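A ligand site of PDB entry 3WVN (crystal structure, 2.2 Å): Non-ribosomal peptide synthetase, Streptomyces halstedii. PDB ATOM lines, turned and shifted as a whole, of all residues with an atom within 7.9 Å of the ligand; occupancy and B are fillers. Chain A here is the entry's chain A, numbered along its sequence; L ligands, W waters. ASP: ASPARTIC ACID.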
ATOM      1  N   ILE A 199      10.806 -27.553   3.749  1.00  0.00           N
ATOM      2  CA  ILE A 199      10.399 -26.182   3.472  1.00  0.00           C
ATOM      3  C   ILE A 199      10.143 -25.572   4.804  1.00  0.00           C
ATOM      4  O   ILE A 199       9.215 -25.967   5.484  1.00  0.00           O
ATOM      5  CB  ILE A 199       9.102 -26.086   2.674  1.00  0.00           C
ATOM      6  CG1 ILE A 199       9.138 -26.908   1.378  1.00  0.00           C
ATOM      7  CG2 ILE A 199       8.772 -24.614   2.357  1.00  0.00           C
ATOM      8  CD1 ILE A 199      10.089 -26.316   0.390  1.00  0.00           C
ATOM      9  N   THR A 201       8.718 -22.871   7.185  1.00  0.00           N
ATOM     10  CA  THR A 201       7.620 -21.878   7.180  1.00  0.00           C
ATOM     11  C   THR A 201       7.688 -20.933   8.384  1.00  0.00           C
ATOM     12  O   THR A 201       7.022 -19.919   8.421  1.00  0.00           O
ATOM     13  CB  THR A 201       6.279 -22.623   7.248  1.00  0.00           C
ATOM     14  OG1 THR A 201       6.293 -23.507   8.392  1.00  0.00           O
ATOM     15  CG2 THR A 201       6.067 -23.480   5.985  1.00  0.00           C
ATOM     16  N   ILE A 225      -1.950 -29.649  -9.633  1.00  0.00           N
ATOM     17  CA  ILE A 225      -2.067 -28.205  -9.893  1.00  0.00           C
ATOM     18  C   ILE A 225      -2.156 -27.980 -11.369  1.00  0.00           C
ATOM     19  O   ILE A 225      -2.982 -27.186 -11.857  1.00  0.00           O
ATOM     20  CB  ILE A 225      -0.877 -27.426  -9.322  1.00  0.00           C
ATOM     21  CG1 ILE A 225      -0.976 -27.387  -7.812  1.00  0.00           C
ATOM     22  CG2 ILE A 225      -0.828 -25.994  -9.889  1.00  0.00           C
ATOM     23  CD1 ILE A 225       0.359 -27.058  -7.087  1.00  0.00           C
ATOM     24  N   TRP A 245      10.378 -20.638  -1.032  1.00  0.00           N
ATOM     25  CA  TRP A 245       8.943 -20.669  -0.780  1.00  0.00           C
ATOM     26  C   TRP A 245       8.420 -21.751  -1.773  1.00  0.00           C
ATOM     27  O   TRP A 245       8.919 -21.834  -2.871  1.00  0.00           O
ATOM     28  CB  TRP A 245       8.422 -19.278  -1.172  1.00  0.00           C
ATOM     29  CG  TRP A 245       7.012 -18.846  -0.888  1.00  0.00           C
ATOM     30  CD1 TRP A 245       5.929 -19.607  -0.471  1.00  0.00           C
ATOM     31  CD2 TRP A 245       6.512 -17.528  -1.120  1.00  0.00           C
ATOM     32  NE1 TRP A 245       4.798 -18.799  -0.374  1.00  0.00           N
ATOM     33  CE2 TRP A 245       5.144 -17.530  -0.771  1.00  0.00           C
ATOM     34  CE3 TRP A 245       7.104 -16.339  -1.543  1.00  0.00           C
ATOM     35  CZ2 TRP A 245       4.360 -16.375  -0.840  1.00  0.00           C
ATOM     36  CZ3 TRP A 245       6.336 -15.187  -1.616  1.00  0.00           C
ATOM     37  CH2 TRP A 245       4.977 -15.211  -1.268  1.00  0.00           C
ATOM     38  N   ASP A 246       7.452 -22.554  -1.400  1.00  0.00           N
ATOM     39  CA  ASP A 246       6.924 -23.550  -2.340  1.00  0.00           C
ATOM     40  C   ASP A 246       6.250 -22.923  -3.565  1.00  0.00           C
ATOM     41  O   ASP A 246       6.043 -23.589  -4.588  1.00  0.00           O
ATOM     42  CB  ASP A 246       6.033 -24.599  -1.640  1.00  0.00           C
ATOM     43  CG  ASP A 246       4.664 -24.072  -1.209  1.00  0.00           C
ATOM     44  OD1 ASP A 246       4.150 -23.034  -1.716  1.00  0.00           O
ATOM     45  OD2 ASP A 246       4.072 -24.774  -0.339  1.00  0.00           O
ATOM     46  N   PHE A 247       5.949 -21.628  -3.492  1.00  0.00           N
ATOM     47  CA  PHE A 247       5.379 -20.930  -4.651  1.00  0.00           C
ATOM     48  C   PHE A 247       6.403 -20.937  -5.751  1.00  0.00           C
ATOM     49  O   PHE A 247       6.159 -21.424  -6.836  1.00  0.00           O
ATOM     50  CB  PHE A 247       4.965 -19.503  -4.270  1.00  0.00           C
ATOM     51  CG  PHE A 247       3.688 -19.062  -4.886  1.00  0.00           C
ATOM     52  CD1 PHE A 247       3.352 -19.435  -6.181  1.00  0.00           C
ATOM     53  CD2 PHE A 247       2.821 -18.271  -4.184  1.00  0.00           C
ATOM     54  CE1 PHE A 247       2.145 -19.029  -6.761  1.00  0.00           C
ATOM     55  CE2 PHE A 247       1.622 -17.844  -4.767  1.00  0.00           C
ATOM     56  CZ  PHE A 247       1.291 -18.194  -6.054  1.00  0.00           C
ATOM     57  N   GLY A 248       7.639 -20.527  -5.474  1.00  0.00           N
ATOM     58  CA  GLY A 248       8.681 -20.651  -6.504  1.00  0.00           C
ATOM     59  C   GLY A 248       9.117 -22.076  -6.865  1.00  0.00           C
ATOM     60  O   GLY A 248       9.412 -22.414  -8.043  1.00  0.00           O
ATOM     61  N   TYR A 250       7.538 -24.777  -6.952  1.00  0.00           N
ATOM     62  CA  TYR A 250       6.589 -25.441  -7.846  1.00  0.00           C
ATOM     63  C   TYR A 250       6.470 -24.834  -9.224  1.00  0.00           C
ATOM     64  O   TYR A 250       6.032 -25.520 -10.144  1.00  0.00           O
ATOM     65  CB  TYR A 250       5.252 -25.608  -7.187  1.00  0.00           C
ATOM     66  CG  TYR A 250       5.233 -26.793  -6.231  1.00  0.00           C
ATOM     67  CD1 TYR A 250       4.605 -27.975  -6.587  1.00  0.00           C
ATOM     68  CD2 TYR A 250       5.813 -26.711  -4.997  1.00  0.00           C
ATOM     69  CE1 TYR A 250       4.547 -29.051  -5.707  1.00  0.00           C
ATOM     70  CE2 TYR A 250       5.789 -27.780  -4.106  1.00  0.00           C
ATOM     71  CZ  TYR A 250       5.139 -28.939  -4.466  1.00  0.00           C
ATOM     72  OH  TYR A 250       5.136 -30.034  -3.648  1.00  0.00           O
ATOM     73  N   LYS A 251       6.919 -23.589  -9.397  1.00  0.00           N
ATOM     74  CA  LYS A 251       7.100 -23.054 -10.749  1.00  0.00           C
ATOM     75  C   LYS A 251       8.333 -23.704 -11.455  1.00  0.00           C
ATOM     76  O   LYS A 251       8.304 -23.972 -12.679  1.00  0.00           O
ATOM     77  CB  LYS A 251       7.021 -21.509 -10.777  1.00  0.00           C
ATOM     78  CG  LYS A 251       5.574 -20.918 -10.416  1.00  0.00           C
ATOM     79  CD  LYS A 251       4.293 -21.881 -10.289  1.00  0.00           C
ATOM     80  CE  LYS A 251       3.857 -22.139  -8.811  1.00  0.00           C
ATOM     81  NZ  LYS A 251       2.455 -22.568  -8.374  1.00  0.00           N
ATOM     82  N   VAL A 288       1.082 -12.728  -5.758  1.00  0.00           N
ATOM     83  CA  VAL A 288       0.554 -12.579  -4.412  1.00  0.00           C
ATOM     84  C   VAL A 288      -0.095 -11.188  -4.379  1.00  0.00           C
ATOM     85  O   VAL A 288       0.204 -10.351  -5.256  1.00  0.00           O
ATOM     86  CB  VAL A 288       1.841 -12.793  -3.531  1.00  0.00           C
ATOM     87  CG1 VAL A 288       2.391 -11.558  -2.877  1.00  0.00           C
ATOM     88  CG2 VAL A 288       1.688 -14.018  -2.639  1.00  0.00           C
ATOM     89  N   ASN A 314      -3.012 -16.639  -8.093  1.00  0.00           N
ATOM     90  CA  ASN A 314      -2.847 -16.027  -6.807  1.00  0.00           C
ATOM     91  C   ASN A 314      -3.095 -17.013  -5.673  1.00  0.00           C
ATOM     92  O   ASN A 314      -4.063 -17.762  -5.667  1.00  0.00           O
ATOM     93  CB  ASN A 314      -3.774 -14.847  -6.629  1.00  0.00           C
ATOM     94  CG  ASN A 314      -3.580 -14.173  -5.282  1.00  0.00           C
ATOM     95  OD1 ASN A 314      -2.708 -13.319  -5.120  1.00  0.00           O
ATOM     96  ND2 ASN A 314      -4.341 -14.614  -4.292  1.00  0.00           N
ATOM     97  N   SER A 315      -2.150 -17.037  -4.732  1.00  0.00           N
ATOM     98  CA  SER A 315      -2.379 -17.736  -3.510  1.00  0.00           C
ATOM     99  C   SER A 315      -1.722 -16.960  -2.395  1.00  0.00           C
ATOM    100  O   SER A 315      -1.249 -15.839  -2.593  1.00  0.00           O
ATOM    101  CB  SER A 315      -1.789 -19.164  -3.567  1.00  0.00           C
ATOM    102  OG  SER A 315      -2.445 -19.987  -2.613  1.00  0.00           O
ATOM    103  N   ALA A 316      -1.660 -17.605  -1.239  1.00  0.00           N
ATOM    104  CA  ALA A 316      -0.976 -17.085  -0.057  1.00  0.00           C
ATOM    105  C   ALA A 316      -1.866 -16.101   0.684  1.00  0.00           C
ATOM    106  O   ALA A 316      -1.823 -16.081   1.912  1.00  0.00           O
ATOM    107  CB  ALA A 316       0.363 -16.473  -0.390  1.00  0.00           C
ATOM    108  N   ALA A 317      -2.661 -15.293  -0.016  1.00  0.00           N
ATOM    109  CA  ALA A 317      -3.538 -14.312   0.654  1.00  0.00           C
ATOM    110  C   ALA A 317      -4.654 -13.895  -0.258  1.00  0.00           C
ATOM    111  O   ALA A 317      -4.637 -14.202  -1.443  1.00  0.00           O
ATOM    112  CB  ALA A 317      -2.769 -13.095   1.155  1.00  0.00           C
ATOM    113  N   MET A 339      -6.561 -19.182  -5.731  1.00  0.00           N
ATOM    114  CA  MET A 339      -6.125 -20.453  -5.160  1.00  0.00           C
ATOM    115  C   MET A 339      -5.948 -20.291  -3.674  1.00  0.00           C
ATOM    116  O   MET A 339      -5.900 -19.188  -3.193  1.00  0.00           O
ATOM    117  CB  MET A 339      -4.799 -20.926  -5.755  1.00  0.00           C
ATOM    118  CG  MET A 339      -4.760 -20.712  -7.266  1.00  0.00           C
ATOM    119  SD  MET A 339      -3.329 -21.410  -8.070  1.00  0.00           S
ATOM    120  CE  MET A 339      -2.061 -20.463  -7.214  1.00  0.00           C
ATOM    121  N   TYR A 340      -5.897 -21.398  -2.954  1.00  0.00           N
ATOM    122  CA  TYR A 340      -5.662 -21.363  -1.522  1.00  0.00           C
ATOM    123  C   TYR A 340      -4.838 -22.598  -1.184  1.00  0.00           C
ATOM    124  O   TYR A 340      -5.093 -23.688  -1.661  1.00  0.00           O
ATOM    125  CB  TYR A 340      -6.994 -21.332  -0.759  1.00  0.00           C
ATOM    126  CG  TYR A 340      -6.984 -21.982   0.610  1.00  0.00           C
ATOM    127  CD1 TYR A 340      -6.241 -21.418   1.660  1.00  0.00           C
ATOM    128  CD2 TYR A 340      -7.740 -23.122   0.868  1.00  0.00           C
ATOM    129  CE1 TYR A 340      -6.269 -21.968   2.910  1.00  0.00           C
ATOM    130  CE2 TYR A 340      -7.773 -23.698   2.134  1.00  0.00           C
ATOM    131  CZ  TYR A 340      -7.024 -23.120   3.149  1.00  0.00           C
ATOM    132  OH  TYR A 340      -7.018 -23.718   4.392  1.00  0.00           O
ATOM    133  N   GLY A 341      -3.861 -22.428  -0.305  1.00  0.00           N
ATOM    134  CA  GLY A 341      -3.071 -23.580   0.098  1.00  0.00           C
ATOM    135  C   GLY A 341      -2.317 -23.351   1.372  1.00  0.00           C
ATOM    136  O   GLY A 341      -2.235 -22.228   1.862  1.00  0.00           O
ATOM    137  N   GLN A 342      -1.751 -24.455   1.862  1.00  0.00           N
ATOM    138  CA  GLN A 342      -0.728 -24.415   2.894  1.00  0.00           C
ATOM    139  C   GLN A 342       0.429 -25.244   2.459  1.00  0.00           C
ATOM    140  O   GLN A 342       0.268 -26.213   1.688  1.00  0.00           O
ATOM    141  CB  GLN A 342      -1.274 -25.025   4.189  1.00  0.00           C
ATOM    142  CG  GLN A 342      -2.413 -24.266   4.771  1.00  0.00           C
ATOM    143  CD  GLN A 342      -2.743 -24.777   6.135  1.00  0.00           C
ATOM    144  OE1 GLN A 342      -2.471 -25.946   6.483  1.00  0.00           O
ATOM    145  NE2 GLN A 342      -3.329 -23.932   6.933  1.00  0.00           N
ATOM    146  N   THR A 343       1.597 -24.951   3.028  1.00  0.00           N
ATOM    147  CA  THR A 343       2.785 -25.658   2.629  1.00  0.00           C
ATOM    148  C   THR A 343       2.646 -27.132   3.039  1.00  0.00           C
ATOM    149  O   THR A 343       3.121 -28.020   2.330  1.00  0.00           O
ATOM    150  CB  THR A 343       4.042 -25.027   3.243  1.00  0.00           C
ATOM    151  OG1 THR A 343       4.206 -23.734   2.691  1.00  0.00           O
ATOM    152  CG2 THR A 343       5.276 -25.847   2.881  1.00  0.00           C
ATOM    153  N   GLU A 344       1.889 -27.369   4.098  1.00  0.00           N
ATOM    154  CA  GLU A 344       1.622 -28.729   4.638  1.00  0.00           C
ATOM    155  C   GLU A 344       1.106 -29.721   3.591  1.00  0.00           C
ATOM    156  O   GLU A 344       1.271 -30.929   3.785  1.00  0.00           O
ATOM    157  CB  GLU A 344       0.593 -28.616   5.753  1.00  0.00           C
ATOM    158  CG  GLU A 344       1.121 -28.128   7.081  1.00  0.00           C
ATOM    159  CD  GLU A 344       1.408 -26.624   7.186  1.00  0.00           C
ATOM    160  OE1 GLU A 344       1.278 -25.846   6.201  1.00  0.00           O
ATOM    161  OE2 GLU A 344       1.852 -26.218   8.281  1.00  0.00           O
ATOM    162  N   CYS A 345       0.422 -29.242   2.545  1.00  0.00           N
ATOM    163  CA  CYS A 345       0.022 -30.114   1.434  1.00  0.00           C
ATOM    164  C   CYS A 345       0.201 -29.432   0.086  1.00  0.00           C
ATOM    165  O   CYS A 345      -0.475 -29.787  -0.881  1.00  0.00           O
ATOM    166  CB  CYS A 345      -1.424 -30.541   1.576  1.00  0.00           C
ATOM    167  SG  CYS A 345      -2.613 -29.199   1.532  1.00  0.00           S
ATOM    168  N   LYS A 346       1.139 -28.456   0.043  1.00  0.00           N
ATOM    169  CA  LYS A 346       1.364 -27.548  -1.092  1.00  0.00           C
ATOM    170  C   LYS A 346       0.195 -26.639  -1.401  1.00  0.00           C
ATOM    171  O   LYS A 346       0.302 -25.446  -1.264  1.00  0.00           O
ATOM    172  CB  LYS A 346       1.800 -28.266  -2.380  1.00  0.00           C
ATOM    173  CG  LYS A 346       1.836 -27.360  -3.632  1.00  0.00           C
ATOM    174  CD  LYS A 346       2.675 -26.056  -3.424  1.00  0.00           C
ATOM    175  CE  LYS A 346       2.542 -25.165  -4.650  1.00  0.00           C
ATOM    176  NZ  LYS A 346       3.284 -23.885  -4.585  1.00  0.00           N
ATOM    177  N   ARG A 347      -0.899 -27.214  -1.867  1.00  0.00           N
ATOM    178  CA  ARG A 347      -2.068 -26.428  -2.233  1.00  0.00           C
ATOM    179  C   ARG A 347      -3.344 -27.210  -1.986  1.00  0.00           C
ATOM    180  O   ARG A 347      -3.328 -28.424  -1.971  1.00  0.00           O
ATOM    181  CB  ARG A 347      -1.933 -25.964  -3.662  1.00  0.00           C
ATOM    182  CG  ARG A 347      -3.043 -25.022  -4.123  1.00  0.00           C
ATOM    183  CD  ARG A 347      -2.636 -24.334  -5.449  1.00  0.00           C
ATOM    184  NE  ARG A 347      -1.541 -23.460  -5.139  1.00  0.00           N
ATOM    185  CZ  ARG A 347      -0.594 -23.075  -5.986  1.00  0.00           C
ATOM    186  NH1 ARG A 347      -0.600 -23.449  -7.250  1.00  0.00           N
ATOM    187  NH2 ARG A 347       0.372 -22.275  -5.541  1.00  0.00           N
ATOM    188  N   ILE A 348      -4.443 -26.504  -1.718  1.00  0.00           N
ATOM    189  CA  ILE A 348      -5.661 -27.129  -1.268  1.00  0.00           C
ATOM    190  C   ILE A 348      -6.794 -26.997  -2.289  1.00  0.00           C
ATOM    191  O   ILE A 348      -7.437 -28.006  -2.629  1.00  0.00           O
ATOM    192  CB  ILE A 348      -6.074 -26.528   0.060  1.00  0.00           C
ATOM    193  CG1 ILE A 348      -5.098 -26.969   1.133  1.00  0.00           C
ATOM    194  CG2 ILE A 348      -7.487 -26.965   0.428  1.00  0.00           C
ATOM    195  CD1 ILE A 348      -5.252 -26.197   2.418  1.00  0.00           C
ATOM    196  N   SER A 349      -6.997 -25.791  -2.795  1.00  0.00           N
ATOM    197  CA  SER A 349      -8.042 -25.537  -3.791  1.00  0.00           C
ATOM    198  C   SER A 349      -7.551 -24.570  -4.848  1.00  0.00           C
ATOM    199  O   SER A 349      -6.751 -23.674  -4.560  1.00  0.00           O
ATOM    200  CB  SER A 349      -9.278 -24.981  -3.117  1.00  0.00           C
ATOM    201  OG  SER A 349      -9.010 -23.676  -2.614  1.00  0.00           O
ATOM    202  N   ILE A 350      -8.062 -24.756  -6.061  1.00  0.00           N
ATOM    203  CA  ILE A 350      -7.916 -23.836  -7.207  1.00  0.00           C
ATOM    204  C   ILE A 350      -9.312 -23.578  -7.811  1.00  0.00           C
ATOM    205  O   ILE A 350     -10.089 -24.535  -8.041  1.00  0.00           O
ATOM    206  CB  ILE A 350      -7.014 -24.432  -8.289  1.00  0.00           C
ATOM    207  CG1 ILE A 350      -5.589 -24.642  -7.720  1.00  0.00           C
ATOM    208  CG2 ILE A 350      -6.966 -23.519  -9.472  1.00  0.00           C
ATOM    209  CD1 ILE A 350      -4.651 -25.289  -8.719  1.00  0.00           C
HETATM  210  N   ASP L   1       1.698 -23.125  -0.364  1.00  0.00           N
HETATM  211  CA  ASP L   1       0.505 -22.302  -0.805  1.00  0.00           C
HETATM  212  C   ASP L   1       0.198 -22.415  -2.289  1.00  0.00           C
HETATM  213  O   ASP L   1       1.149 -22.593  -3.108  1.00  0.00           O
HETATM  214  CB  ASP L   1       0.672 -20.825  -0.453  1.00  0.00           C
HETATM  215  CG  ASP L   1       1.216 -20.607   1.008  1.00  0.00           C
HETATM  216  OD1 ASP L   1       1.553 -19.450   1.333  1.00  0.00           O
HETATM  217  OD2 ASP L   1       1.324 -21.595   1.796  1.00  0.00           O
HETATM  218  OXT ASP L   1      -1.003 -22.310  -2.654  1.00  0.00           O
HETATM  219  O   HOH W   1       3.456 -18.220   3.050  1.00  0.00           O
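The side-chain amino group (NZ) of Lys 346 is in salt-bridge range of an oxygen (O) of the ligand (2.9 Å).
The side-chain hydroxyl (OG) of Ser 315 lies within hydrogen-bond range of an oxygen (OXT) of the ligand (2.7 Å).
A nitrogen (N) of the ligand is in hydrogen-bond range of the backbone carbonyl oxygen (O) of Lys 346.
NH2 of Arg 347 lies within salt-bridge range of O of the ligand, at 2.6 Å.
N of the ligand is in salt-bridge range of OD1 of Asp 246.
Merely in contact with the ligand: Thr 343, Gly 341, Ala 316, Gln 342 and Trp 245.
Hydrophobic or aromatic side chains that line the ligand: Ala 316.
The nearest printed residue that does not touch the ligand is Tyr 340 (4.1 Å).
The guanidinium group (NH1) of Arg 347 sits close to the side-chain sulfur (SD) of Met 339, 3.5 Å away.
The side-chain hydroxyl (OG1) of Thr 343 is in hydrogen-bond range of the side-chain carboxylate (OD2) of Asp 246 (3.2 Å).
The side-chain carboxylate of Asp 246 lies within salt-bridge range of the side-chain amino group of Lys 346, at 3.1 Å.
The backbone carbonyl oxygen (O) of Arg 347 is in hydrogen-bond range of the side-chain sulfur (SG) of Cys 345, 3.7 Å away.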
